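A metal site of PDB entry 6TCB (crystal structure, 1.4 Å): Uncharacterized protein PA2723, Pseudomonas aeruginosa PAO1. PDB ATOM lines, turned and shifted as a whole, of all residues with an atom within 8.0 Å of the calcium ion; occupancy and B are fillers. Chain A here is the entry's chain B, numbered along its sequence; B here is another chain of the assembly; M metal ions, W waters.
The calcium ion is bound by the side-chain carboxylate (OD2) of Asp 68 of chain B (2.2 Å), water W2 (2.3 Å), water W1 (2.3 Å), the side-chain carboxylate (OD2) of Asp 66 of chain A (2.5 Å), the side-chain carboxylate (OD2) of Asp 68 of chain A (2.5 Å) and the side-chain carboxylate (OD1) of Asp 66 of chain A (2.5 Å).
The side-chain carboxylate (OD1) of Asp 66 of chain A sits close to the backbone NH (N) of Ala 69 of chain A. The side-chain carboxylate (OD1) of Asp 68 of chain B lies within salt-bridge range of the guanidinium group (NH2) of Arg 71 of chain B, at 2.9 Å. The side-chain carboxylate (OD1) of Asp 66 of chain B sits at hydrogen-bond distance from the backbone NH (N) of Asp 68 of chain B. OD1 of Asp 68 of chain B lies within hydrogen-bond range of N of Leu 67 of chain A (2.9 Å). The side-chain carboxylate (OD1) of Asp 68 of chain A lies within hydrogen-bond range of the backbone NH (N) of Leu 67 of chain B, at 2.8 Å.
The nearest printed residue that does not touch the calcium ion is Asp 66 of chain B (4.4 Å).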
ATOM      1  N   CYS A  65       4.448 -20.023 -16.788  1.00  0.00           N
ATOM      2  CA  CYS A  65       3.470 -20.135 -17.859  1.00  0.00           C
ATOM      3  C   CYS A  65       2.211 -20.797 -17.285  1.00  0.00           C
ATOM      4  O   CYS A  65       2.310 -21.831 -16.611  1.00  0.00           O
ATOM      5  CB  CYS A  65       4.031 -20.985 -19.002  1.00  0.00           C
ATOM      6  SG  CYS A  65       2.942 -21.145 -20.438  1.00  0.00           S
ATOM      7  N   ASP A  66       1.060 -20.222 -17.592  1.00  0.00           N
ATOM      8  CA  ASP A  66      -0.197 -20.614 -16.963  1.00  0.00           C
ATOM      9  C   ASP A  66      -0.687 -21.936 -17.553  1.00  0.00           C
ATOM     10  O   ASP A  66      -0.970 -22.025 -18.750  1.00  0.00           O
ATOM     11  CB  ASP A  66      -1.199 -19.496 -17.190  1.00  0.00           C
ATOM     12  CG  ASP A  66      -2.440 -19.639 -16.347  1.00  0.00           C
ATOM     13  OD1 ASP A  66      -3.111 -20.684 -16.431  1.00  0.00           O
ATOM     14  OD2 ASP A  66      -2.742 -18.699 -15.575  1.00  0.00           O
ATOM     15  N   LEU A  67      -0.841 -22.953 -16.696  1.00  0.00           N
ATOM     16  CA  LEU A  67      -1.207 -24.272 -17.222  1.00  0.00           C
ATOM     17  C   LEU A  67      -2.662 -24.315 -17.677  1.00  0.00           C
ATOM     18  O   LEU A  67      -3.000 -25.086 -18.582  1.00  0.00           O
ATOM     19  CB  LEU A  67      -0.997 -25.326 -16.149  1.00  0.00           C
ATOM     20  CG  LEU A  67       0.434 -25.824 -15.954  1.00  0.00           C
ATOM     21  CD1 LEU A  67       0.551 -26.530 -14.633  1.00  0.00           C
ATOM     22  CD2 LEU A  67       0.837 -26.735 -17.106  1.00  0.00           C
ATOM     23  N   ASP A  68      -3.533 -23.524 -17.042  1.00  0.00           N
ATOM     24  CA  ASP A  68      -4.915 -23.454 -17.496  1.00  0.00           C
ATOM     25  C   ASP A  68      -4.981 -22.850 -18.886  1.00  0.00           C
ATOM     26  O   ASP A  68      -5.763 -23.312 -19.734  1.00  0.00           O
ATOM     27  CB  ASP A  68      -5.725 -22.659 -16.485  1.00  0.00           C
ATOM     28  CG  ASP A  68      -5.579 -23.206 -15.076  1.00  0.00           C
ATOM     29  OD1 ASP A  68      -6.153 -24.285 -14.790  1.00  0.00           O
ATOM     30  OD2 ASP A  68      -4.830 -22.614 -14.255  1.00  0.00           O
ATOM     31  N   ALA A  69      -4.159 -21.833 -19.149  1.00  0.00           N
ATOM     32  CA  ALA A  69      -4.096 -21.277 -20.493  1.00  0.00           C
ATOM     33  C   ALA A  69      -3.581 -22.299 -21.493  1.00  0.00           C
ATOM     34  O   ALA A  69      -4.044 -22.356 -22.636  1.00  0.00           O
ATOM     35  CB  ALA A  69      -3.242 -20.006 -20.500  1.00  0.00           C
ATOM     36  N   VAL A  70      -2.607 -23.121 -21.085  1.00  0.00           N
ATOM     37  CA  VAL A  70      -2.101 -24.151 -21.998  1.00  0.00           C
ATOM     38  C   VAL A  70      -3.186 -25.178 -22.304  1.00  0.00           C
ATOM     39  O   VAL A  70      -3.339 -25.624 -23.448  1.00  0.00           O
ATOM     40  CB  VAL A  70      -0.832 -24.808 -21.421  1.00  0.00           C
ATOM     41  CG1 VAL A  70      -0.433 -25.975 -22.290  1.00  0.00           C
ATOM     42  CG2 VAL A  70       0.320 -23.810 -21.318  1.00  0.00           C
ATOM     43  N   ASP B  66      -8.269 -26.477 -10.848  1.00  0.00           N
ATOM     44  CA  ASP B  66      -7.319 -25.506 -11.360  1.00  0.00           C
ATOM     45  C   ASP B  66      -5.953 -26.148 -11.529  1.00  0.00           C
ATOM     46  O   ASP B  66      -5.376 -26.656 -10.567  1.00  0.00           O
ATOM     47  CB  ASP B  66      -7.253 -24.322 -10.408  1.00  0.00           C
ATOM     48  CG  ASP B  66      -6.452 -23.197 -10.979  1.00  0.00           C
ATOM     49  OD1 ASP B  66      -5.221 -23.228 -10.851  1.00  0.00           O
ATOM     50  OD2 ASP B  66      -7.053 -22.282 -11.599  1.00  0.00           O
ATOM     51  N   LEU B  67      -5.405 -26.081 -12.740  1.00  0.00           N
ATOM     52  CA  LEU B  67      -4.152 -26.772 -13.013  1.00  0.00           C
ATOM     53  C   LEU B  67      -2.969 -26.087 -12.333  1.00  0.00           C
ATOM     54  O   LEU B  67      -2.033 -26.764 -11.892  1.00  0.00           O
ATOM     55  CB  LEU B  67      -3.905 -26.875 -14.510  1.00  0.00           C
ATOM     56  CG  LEU B  67      -4.918 -27.680 -15.310  1.00  0.00           C
ATOM     57  CD1 LEU B  67      -4.528 -27.715 -16.790  1.00  0.00           C
ATOM     58  CD2 LEU B  67      -5.056 -29.082 -14.804  1.00  0.00           C
ATOM     59  N   ASP B  68      -2.987 -24.752 -12.256  1.00  0.00           N
ATOM     60  CA  ASP B  68      -1.910 -24.071 -11.548  1.00  0.00           C
ATOM     61  C   ASP B  68      -1.885 -24.465 -10.077  1.00  0.00           C
ATOM     62  O   ASP B  68      -0.809 -24.590  -9.474  1.00  0.00           O
ATOM     63  CB  ASP B  68      -2.037 -22.562 -11.728  1.00  0.00           C
ATOM     64  CG  ASP B  68      -1.624 -22.093 -13.120  1.00  0.00           C
ATOM     65  OD1 ASP B  68      -0.830 -22.775 -13.800  1.00  0.00           O
ATOM     66  OD2 ASP B  68      -2.105 -21.015 -13.540  1.00  0.00           O
ATOM     67  N   ALA B  69      -3.057 -24.708  -9.490  1.00  0.00           N
ATOM     68  CA  ALA B  69      -3.108 -25.141  -8.107  1.00  0.00           C
ATOM     69  C   ALA B  69      -2.556 -26.552  -7.949  1.00  0.00           C
ATOM     70  O   ALA B  69      -1.887 -26.844  -6.953  1.00  0.00           O
ATOM     71  CB  ALA B  69      -4.546 -25.059  -7.587  1.00  0.00           C
ATOM     72  N   ARG B  71      -0.151 -27.808  -9.849  1.00  0.00           N
ATOM     73  CA  ARG B  71       1.294 -27.625  -9.926  1.00  0.00           C
ATOM     74  C   ARG B  71       1.861 -27.086  -8.613  1.00  0.00           C
ATOM     75  O   ARG B  71       2.895 -27.559  -8.140  1.00  0.00           O
ATOM     76  CB  ARG B  71       1.656 -26.707 -11.099  1.00  0.00           C
ATOM     77  CG  ARG B  71       3.139 -26.390 -11.165  1.00  0.00           C
ATOM     78  CD  ARG B  71       3.561 -25.707 -12.468  1.00  0.00           C
ATOM     79  NE  ARG B  71       2.772 -24.510 -12.726  1.00  0.00           N
ATOM     80  CZ  ARG B  71       2.866 -23.757 -13.826  1.00  0.00           C
ATOM     81  NH1 ARG B  71       3.724 -24.053 -14.791  1.00  0.00           N
ATOM     82  NH2 ARG B  71       2.074 -22.708 -13.942  1.00  0.00           N
HETATM   83 CA    CA M   1      -4.088 -20.211 -14.143  1.00  0.00          CA
HETATM   84  O   HOH W   1      -3.902 -18.269 -12.944  1.00  0.00           O
HETATM   85  O   HOH W   2      -6.039 -19.498 -15.041  1.00  0.00           O
